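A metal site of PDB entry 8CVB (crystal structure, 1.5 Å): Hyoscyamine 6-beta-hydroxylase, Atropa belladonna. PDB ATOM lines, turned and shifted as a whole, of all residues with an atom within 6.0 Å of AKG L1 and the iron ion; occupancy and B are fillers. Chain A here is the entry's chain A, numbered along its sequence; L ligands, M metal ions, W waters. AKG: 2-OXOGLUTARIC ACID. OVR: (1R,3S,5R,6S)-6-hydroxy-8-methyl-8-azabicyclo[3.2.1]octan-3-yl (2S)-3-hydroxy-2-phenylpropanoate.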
ATOM      1  N   LEU A 198     -33.376  21.049  -6.789  1.00  0.00           N
ATOM      2  CA  LEU A 198     -32.017  20.486  -6.851  1.00  0.00           C
ATOM      3  C   LEU A 198     -32.009  19.191  -6.043  1.00  0.00           C
ATOM      4  O   LEU A 198     -32.195  19.257  -4.809  1.00  0.00           O
ATOM      5  CB  LEU A 198     -31.018  21.509  -6.281  1.00  0.00           C
ATOM      6  CG  LEU A 198     -30.519  22.557  -7.263  1.00  0.00           C
ATOM      7  CD1 LEU A 198     -31.660  23.403  -7.798  1.00  0.00           C
ATOM      8  CD2 LEU A 198     -29.448  23.431  -6.610  1.00  0.00           C
ATOM      9  N   ASN A 200     -29.602  16.522  -4.805  1.00  0.00           N
ATOM     10  CA  ASN A 200     -28.145  16.460  -4.556  1.00  0.00           C
ATOM     11  C   ASN A 200     -27.753  15.025  -4.208  1.00  0.00           C
ATOM     12  O   ASN A 200     -28.347  14.466  -3.287  1.00  0.00           O
ATOM     13  CB  ASN A 200     -27.740  17.388  -3.420  1.00  0.00           C
ATOM     14  CG  ASN A 200     -28.171  18.823  -3.694  1.00  0.00           C
ATOM     15  OD1 ASN A 200     -27.789  19.398  -4.704  1.00  0.00           O
ATOM     16  ND2 ASN A 200     -28.954  19.389  -2.792  1.00  0.00           N
ATOM     17  N   TYR A 202     -24.520  12.800  -2.992  1.00  0.00           N
ATOM     18  CA  TYR A 202     -23.190  12.772  -2.346  1.00  0.00           C
ATOM     19  C   TYR A 202     -22.732  11.330  -2.265  1.00  0.00           C
ATOM     20  O   TYR A 202     -23.137  10.592  -1.356  1.00  0.00           O
ATOM     21  CB  TYR A 202     -23.274  13.433  -0.965  1.00  0.00           C
ATOM     22  CG  TYR A 202     -23.917  14.789  -0.955  1.00  0.00           C
ATOM     23  CD1 TYR A 202     -23.180  15.940  -1.195  1.00  0.00           C
ATOM     24  CD2 TYR A 202     -25.275  14.934  -0.720  1.00  0.00           C
ATOM     25  CE1 TYR A 202     -23.773  17.197  -1.188  1.00  0.00           C
ATOM     26  CE2 TYR A 202     -25.876  16.178  -0.705  1.00  0.00           C
ATOM     27  CZ  TYR A 202     -25.124  17.310  -0.939  1.00  0.00           C
ATOM     28  OH  TYR A 202     -25.724  18.540  -0.920  1.00  0.00           O
ATOM     29  N   SER A 214     -20.675  20.136  -0.169  1.00  0.00           N
ATOM     30  CA  SER A 214     -21.171  21.479  -0.565  1.00  0.00           C
ATOM     31  C   SER A 214     -20.428  22.514   0.281  1.00  0.00           C
ATOM     32  O   SER A 214     -20.489  22.420   1.510  1.00  0.00           O
ATOM     33  CB  SER A 214     -22.667  21.559  -0.382  1.00  0.00           C
ATOM     34  OG  SER A 214     -23.227  22.583  -1.193  1.00  0.00           O
ATOM     35  N   HIS A 217     -22.240  28.227   2.164  1.00  0.00           N
ATOM     36  CA  HIS A 217     -22.974  29.202   1.318  1.00  0.00           C
ATOM     37  C   HIS A 217     -24.268  29.634   2.011  1.00  0.00           C
ATOM     38  O   HIS A 217     -24.841  28.828   2.776  1.00  0.00           O
ATOM     39  CB  HIS A 217     -23.270  28.623  -0.071  1.00  0.00           C
ATOM     40  CG  HIS A 217     -24.216  27.457  -0.051  1.00  0.00           C
ATOM     41  ND1 HIS A 217     -23.818  26.192   0.306  1.00  0.00           N
ATOM     42  CD2 HIS A 217     -25.541  27.386  -0.316  1.00  0.00           C
ATOM     43  CE1 HIS A 217     -24.857  25.372   0.245  1.00  0.00           C
ATOM     44  NE2 HIS A 217     -25.924  26.082  -0.145  1.00  0.00           N
ATOM     45  N   TYR A 218     -24.718  30.843   1.710  1.00  0.00           N
ATOM     46  CA  TYR A 218     -26.164  31.184   1.689  1.00  0.00           C
ATOM     47  C   TYR A 218     -26.748  30.610   0.402  1.00  0.00           C
ATOM     48  O   TYR A 218     -26.049  30.625  -0.634  1.00  0.00           O
ATOM     49  CB  TYR A 218     -26.437  32.681   1.601  1.00  0.00           C
ATOM     50  CG  TYR A 218     -26.008  33.537   2.767  1.00  0.00           C
ATOM     51  CD1 TYR A 218     -26.808  33.681   3.889  1.00  0.00           C
ATOM     52  CD2 TYR A 218     -24.837  34.265   2.708  1.00  0.00           C
ATOM     53  CE1 TYR A 218     -26.428  34.498   4.935  1.00  0.00           C
ATOM     54  CE2 TYR A 218     -24.445  35.090   3.753  1.00  0.00           C
ATOM     55  CZ  TYR A 218     -25.248  35.211   4.873  1.00  0.00           C
ATOM     56  OH  TYR A 218     -24.874  36.025   5.907  1.00  0.00           O
ATOM     57  N   ASP A 219     -28.000  30.179   0.446  1.00  0.00           N
ATOM     58  CA  ASP A 219     -28.820  30.046  -0.780  1.00  0.00           C
ATOM     59  C   ASP A 219     -29.108  31.482  -1.248  1.00  0.00           C
ATOM     60  O   ASP A 219     -29.525  32.296  -0.421  1.00  0.00           O
ATOM     61  CB  ASP A 219     -30.084  29.233  -0.531  1.00  0.00           C
ATOM     62  CG  ASP A 219     -29.844  27.752  -0.242  1.00  0.00           C
ATOM     63  OD1 ASP A 219     -28.683  27.298  -0.401  1.00  0.00           O
ATOM     64  OD2 ASP A 219     -30.812  27.067   0.125  1.00  0.00           O
ATOM     65  N   THR A 224     -35.574  28.362   0.878  1.00  0.00           N
ATOM     66  CA  THR A 224     -35.346  26.973   0.414  1.00  0.00           C
ATOM     67  C   THR A 224     -35.965  26.017   1.417  1.00  0.00           C
ATOM     68  O   THR A 224     -35.785  26.233   2.628  1.00  0.00           O
ATOM     69  CB  THR A 224     -33.852  26.685   0.272  1.00  0.00           C
ATOM     70  OG1 THR A 224     -33.330  27.599  -0.696  1.00  0.00           O
ATOM     71  CG2 THR A 224     -33.574  25.252  -0.142  1.00  0.00           C
ATOM     72  N   LEU A 226     -35.685  22.015   2.334  1.00  0.00           N
ATOM     73  CA  LEU A 226     -34.683  20.957   2.130  1.00  0.00           C
ATOM     74  C   LEU A 226     -35.181  19.681   2.819  1.00  0.00           C
ATOM     75  O   LEU A 226     -35.545  19.752   4.005  1.00  0.00           O
ATOM     76  CB  LEU A 226     -33.360  21.465   2.700  1.00  0.00           C
ATOM     77  CG  LEU A 226     -32.199  20.483   2.744  1.00  0.00           C
ATOM     78  CD1 LEU A 226     -31.849  19.996   1.342  1.00  0.00           C
ATOM     79  CD2 LEU A 226     -30.999  21.142   3.405  1.00  0.00           C
ATOM     80  N   GLN A 228     -34.124  15.805   3.865  1.00  0.00           N
ATOM     81  CA  GLN A 228     -32.937  14.943   4.098  1.00  0.00           C
ATOM     82  C   GLN A 228     -33.323  13.758   4.992  1.00  0.00           C
ATOM     83  O   GLN A 228     -34.250  13.910   5.814  1.00  0.00           O
ATOM     84  CB  GLN A 228     -31.792  15.743   4.727  1.00  0.00           C
ATOM     85  CG  GLN A 228     -32.171  16.404   6.039  1.00  0.00           C
ATOM     86  CD  GLN A 228     -30.974  16.876   6.837  1.00  0.00           C
ATOM     87  OE1 GLN A 228     -29.831  16.682   6.456  1.00  0.00           O
ATOM     88  NE2 GLN A 228     -31.247  17.527   7.953  1.00  0.00           N
ATOM     89  N   GLY A 232     -25.107  15.105   7.495  1.00  0.00           N
ATOM     90  CA  GLY A 232     -24.127  15.739   6.594  1.00  0.00           C
ATOM     91  C   GLY A 232     -24.317  17.237   6.489  1.00  0.00           C
ATOM     92  O   GLY A 232     -23.338  17.923   6.183  1.00  0.00           O
ATOM     93  N   LEU A 233     -25.547  17.722   6.707  1.00  0.00           N
ATOM     94  CA  LEU A 233     -25.841  19.178   6.667  1.00  0.00           C
ATOM     95  C   LEU A 233     -25.324  19.826   7.949  1.00  0.00           C
ATOM     96  O   LEU A 233     -25.615  19.315   9.049  1.00  0.00           O
ATOM     97  CB  LEU A 233     -27.351  19.388   6.510  1.00  0.00           C
ATOM     98  CG  LEU A 233     -27.813  20.844   6.520  1.00  0.00           C
ATOM     99  CD1 LEU A 233     -27.239  21.625   5.338  1.00  0.00           C
ATOM    100  CD2 LEU A 233     -29.335  20.908   6.520  1.00  0.00           C
ATOM    101  N   ASN A 255     -34.323  27.018   4.992  1.00  0.00           N
ATOM    102  CA  ASN A 255     -33.110  27.870   4.890  1.00  0.00           C
ATOM    103  C   ASN A 255     -33.541  29.229   4.325  1.00  0.00           C
ATOM    104  O   ASN A 255     -33.994  29.256   3.175  1.00  0.00           O
ATOM    105  CB  ASN A 255     -32.035  27.263   3.978  1.00  0.00           C
ATOM    106  CG  ASN A 255     -31.247  26.126   4.616  1.00  0.00           C
ATOM    107  OD1 ASN A 255     -30.834  26.234   5.762  1.00  0.00           O
ATOM    108  ND2 ASN A 255     -30.988  25.072   3.865  1.00  0.00           N
ATOM    109  N   HIS A 273     -24.739  27.434   5.365  1.00  0.00           N
ATOM    110  CA  HIS A 273     -24.704  25.972   5.577  1.00  0.00           C
ATOM    111  C   HIS A 273     -23.730  25.319   4.594  1.00  0.00           C
ATOM    112  O   HIS A 273     -23.392  25.931   3.565  1.00  0.00           O
ATOM    113  CB  HIS A 273     -26.118  25.378   5.499  1.00  0.00           C
ATOM    114  CG  HIS A 273     -26.838  25.741   4.247  1.00  0.00           C
ATOM    115  ND1 HIS A 273     -27.562  26.914   4.118  1.00  0.00           N
ATOM    116  CD2 HIS A 273     -26.943  25.098   3.057  1.00  0.00           C
ATOM    117  CE1 HIS A 273     -28.082  26.973   2.907  1.00  0.00           C
ATOM    118  NE2 HIS A 273     -27.722  25.864   2.237  1.00  0.00           N
ATOM    119  N   ARG A 274     -23.310  24.108   4.922  1.00  0.00           N
ATOM    120  CA  ARG A 274     -22.400  23.283   4.092  1.00  0.00           C
ATOM    121  C   ARG A 274     -22.809  21.816   4.256  1.00  0.00           C
ATOM    122  O   ARG A 274     -23.609  21.511   5.171  1.00  0.00           O
ATOM    123  CB  ARG A 274     -20.942  23.501   4.509  1.00  0.00           C
ATOM    124  CG  ARG A 274     -20.563  22.799   5.812  1.00  0.00           C
ATOM    125  CD  ARG A 274     -19.146  23.116   6.226  1.00  0.00           C
ATOM    126  NE  ARG A 274     -18.833  22.432   7.471  1.00  0.00           N
ATOM    127  CZ  ARG A 274     -17.749  22.648   8.204  1.00  0.00           C
ATOM    128  NH1 ARG A 274     -16.846  23.530   7.822  1.00  0.00           N
ATOM    129  NH2 ARG A 274     -17.566  21.956   9.325  1.00  0.00           N
ATOM    130  N   VAL A 275     -22.268  20.955   3.410  1.00  0.00           N
ATOM    131  CA  VAL A 275     -22.486  19.492   3.503  1.00  0.00           C
ATOM    132  C   VAL A 275     -21.119  18.811   3.528  1.00  0.00           C
ATOM    133  O   VAL A 275     -20.289  19.112   2.647  1.00  0.00           O
ATOM    134  CB  VAL A 275     -23.373  18.962   2.368  1.00  0.00           C
ATOM    135  CG1 VAL A 275     -23.600  17.461   2.492  1.00  0.00           C
ATOM    136  CG2 VAL A 275     -24.698  19.703   2.309  1.00  0.00           C
ATOM    137  N   ARG A 283     -25.612   9.725   0.068  1.00  0.00           N
ATOM    138  CA  ARG A 283     -26.653  10.596   0.667  1.00  0.00           C
ATOM    139  C   ARG A 283     -27.352  11.329  -0.471  1.00  0.00           C
ATOM    140  O   ARG A 283     -26.651  11.819  -1.378  1.00  0.00           O
ATOM    141  CB  ARG A 283     -26.024  11.571   1.665  1.00  0.00           C
ATOM    142  CG  ARG A 283     -27.005  12.591   2.230  1.00  0.00           C
ATOM    143  CD  ARG A 283     -26.366  13.374   3.368  1.00  0.00           C
ATOM    144  NE  ARG A 283     -27.275  14.364   3.941  1.00  0.00           N
ATOM    145  CZ  ARG A 283     -27.496  15.570   3.436  1.00  0.00           C
ATOM    146  NH1 ARG A 283     -26.887  15.966   2.340  1.00  0.00           N
ATOM    147  NH2 ARG A 283     -28.343  16.382   4.038  1.00  0.00           N
ATOM    148  N   SER A 285     -30.227  14.479  -0.954  1.00  0.00           N
ATOM    149  CA  SER A 285     -31.085  15.555  -0.402  1.00  0.00           C
ATOM    150  C   SER A 285     -31.875  16.198  -1.529  1.00  0.00           C
ATOM    151  O   SER A 285     -31.417  16.152  -2.693  1.00  0.00           O
ATOM    152  CB  SER A 285     -30.294  16.575   0.369  1.00  0.00           C
ATOM    153  OG  SER A 285     -29.484  17.350  -0.504  1.00  0.00           O
ATOM    154  N   ALA A 287     -33.558  19.798  -2.422  1.00  0.00           N
ATOM    155  CA  ALA A 287     -33.636  21.242  -2.105  1.00  0.00           C
ATOM    156  C   ALA A 287     -34.582  21.912  -3.104  1.00  0.00           C
ATOM    157  O   ALA A 287     -34.337  21.798  -4.310  1.00  0.00           O
ATOM    158  CB  ALA A 287     -32.267  21.856  -2.150  1.00  0.00           C
ATOM    159  N   LEU A 289     -35.542  25.454  -4.142  1.00  0.00           N
ATOM    160  CA  LEU A 289     -35.035  26.836  -4.046  1.00  0.00           C
ATOM    161  C   LEU A 289     -36.056  27.758  -4.723  1.00  0.00           C
ATOM    162  O   LEU A 289     -36.148  27.723  -5.961  1.00  0.00           O
ATOM    163  CB  LEU A 289     -33.664  26.936  -4.728  1.00  0.00           C
ATOM    164  CG  LEU A 289     -32.474  26.423  -3.908  1.00  0.00           C
ATOM    165  CD1 LEU A 289     -32.478  24.910  -3.777  1.00  0.00           C
ATOM    166  CD2 LEU A 289     -31.170  26.904  -4.529  1.00  0.00           C
HETATM  167  C1  AKG L   1     -28.602  23.111  -1.395  1.00  0.00           C
HETATM  168  O1  AKG L   1     -28.513  24.346  -1.525  1.00  0.00           O
HETATM  169  O2  AKG L   1     -29.034  22.382  -2.299  1.00  0.00           O
HETATM  170  C2  AKG L   1     -28.214  22.596  -0.259  1.00  0.00           C
HETATM  171  O5  AKG L   1     -27.692  23.338   0.580  1.00  0.00           O
HETATM  172  C3  AKG L   1     -28.364  21.128   0.074  1.00  0.00           C
HETATM  173  C4  AKG L   1     -27.917  20.752   1.475  1.00  0.00           C
HETATM  174  C5  AKG L   1     -27.998  19.282   1.809  1.00  0.00           C
HETATM  175  O3  AKG L   1     -28.446  18.955   2.935  1.00  0.00           O
HETATM  176  O4  AKG L   1     -27.591  18.456   0.966  1.00  0.00           O
HETATM  177  C1  OVR L   2     -26.318  25.315  -5.533  1.00  0.00           C
HETATM  178  C2  OVR L   2     -26.210  26.092  -6.842  1.00  0.00           C
HETATM  179  C3  OVR L   2     -26.158  27.588  -6.625  1.00  0.00           C
HETATM  180  C4  OVR L   2     -25.378  27.994  -5.400  1.00  0.00           C
HETATM  181  C5  OVR L   2     -25.587  27.040  -4.227  1.00  0.00           C
HETATM  182  C6  OVR L   2     -27.036  26.819  -3.786  1.00  0.00           C
HETATM  183  N1  OVR L   2     -25.168  25.698  -4.665  1.00  0.00           N
HETATM  184  C7  OVR L   2     -27.527  25.673  -4.684  1.00  0.00           C
HETATM  185  O1  OVR L   2     -27.912  24.539  -3.915  1.00  0.00           O
HETATM  186  C8  OVR L   2     -24.884  24.768  -3.563  1.00  0.00           C
HETATM  187  O2  OVR L   2     -27.524  28.093  -6.467  1.00  0.00           O
HETATM  188  C9  OVR L   2     -28.257  28.298  -7.583  1.00  0.00           C
HETATM  189  C10 OVR L   2     -29.575  28.972  -7.281  1.00  0.00           C
HETATM  190  C11 OVR L   2     -29.438  30.470  -7.479  1.00  0.00           C
HETATM  191  C12 OVR L   2     -28.883  30.991  -8.645  1.00  0.00           C
HETATM  192  C13 OVR L   2     -28.778  32.362  -8.822  1.00  0.00           C
HETATM  193  C14 OVR L   2     -29.242  33.232  -7.864  1.00  0.00           C
HETATM  194  C15 OVR L   2     -29.801  32.730  -6.709  1.00  0.00           C
HETATM  195  C16 OVR L   2     -29.900  31.363  -6.519  1.00  0.00           C
HETATM  196  C17 OVR L   2     -30.698  28.363  -8.094  1.00  0.00           C
HETATM  197  O3  OVR L   2     -31.900  29.087  -7.857  1.00  0.00           O
HETATM  198  O4  OVR L   2     -27.907  27.976  -8.684  1.00  0.00           O
HETATM  199 FE    FE M   1     -27.947  25.437   0.171  1.00  0.00          FE
HETATM  200  O   HOH W   1     -25.476  21.319  -1.959  1.00  0.00           O
HETATM  201  O   HOH W   2     -30.294  24.711   1.040  1.00  0.00           O
HETATM  202  O   HOH W   3     -26.681  21.946  -4.525  1.00  0.00           O
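The iron ion is bound by the side-chain carboxylate (OD1) of Asp 219 (2.1 Å), an oxygen (O1) of AKG L1 (2.1 Å), a ring nitrogen (NE2) of His 273 (2.1 Å), a ring nitrogen (NE2) of His 217 (2.1 Å) and an oxygen (O5) of AKG L1 (2.2 Å). The iron ion has five donor atoms within binding distance. Slightly farther from the iron ion lies water W2 (2.6 Å).
Residues that only touch AKG L1: Leu 226 (3.4 Å), Leu 233 (3.8 Å), Val 275 (3.4 Å) and Ala 287 (3.3 Å). Hydrophobic or aromatic side chains within 4 Å of AKG L1: Tyr 202, His 217, Leu 226, Leu 233, His 273, Val 275 and Ala 287. Within 4 Å of AKG L1: Asn 200, Tyr 202, His 217, Asp 219, Leu 226, Leu 233, His 273, Val 275, Arg 283, Ser 285 and Ala 287. Along chain A the residues within 4 Å of AKG L1 span positions 200 to 287.
OD2 of Asp 219 sits at hydrogen-bond distance from OG1 of Thr 224, 2.7 Å away. The backbone carbonyl oxygen of Ser 285 is in hydrogen-bond range of the backbone NH of Asn 200 (2.8 Å). The backbone NH (N) of Tyr 202 is in hydrogen-bond range of the backbone carbonyl oxygen (O) of Arg 283, at 2.8 Å. The side-chain amide oxygen (OE1) of Gln 228 is in hydrogen-bond range of the guanidinium group (NH2) of Arg 283, 2.9 Å away. The backbone carbonyl oxygen of Ala 287 sits at hydrogen-bond distance from the backbone NH of Leu 198. N of Val 275 is in hydrogen-bond range of O of Ser 214, at 3.0 Å.
Within 4 Å of the iron ion: His 217, Asp 219 and His 273.
O2 of AKG L1 sits at hydrogen-bond distance from O1 of OVR L2 (2.9 Å).
Water W2 bridges the side-chain carboxylate (OD2) of Asp 219 and the side-chain amide nitrogen (ND2) of Asn 255. Water W3 lies within hydrogen-bond range of the side-chain amide oxygen (OD1) of Asn 200 (2.8 Å), an oxygen (O1) of OVR L2 (2.9 Å) and an oxygen (O2) of AKG L1 (3.3 Å). Water W1 lies within hydrogen-bond range of OG of Ser 214 (2.7 Å) and OH of Tyr 202 (3.0 Å).
An oxygen (O4) of AKG L1 is in hydrogen-bond range of the side-chain hydroxyl (OG) of Ser 285, at 2.6 Å. O4 of AKG L1 is in hydrogen-bond range of OH of Tyr 202 (2.7 Å). An oxygen (O3) of AKG L1 is in salt-bridge range of the guanidinium group of Arg 283 (2.8 Å). O2 of AKG L1 sits at hydrogen-bond distance from ND2 of Asn 200, 3.0 Å away.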
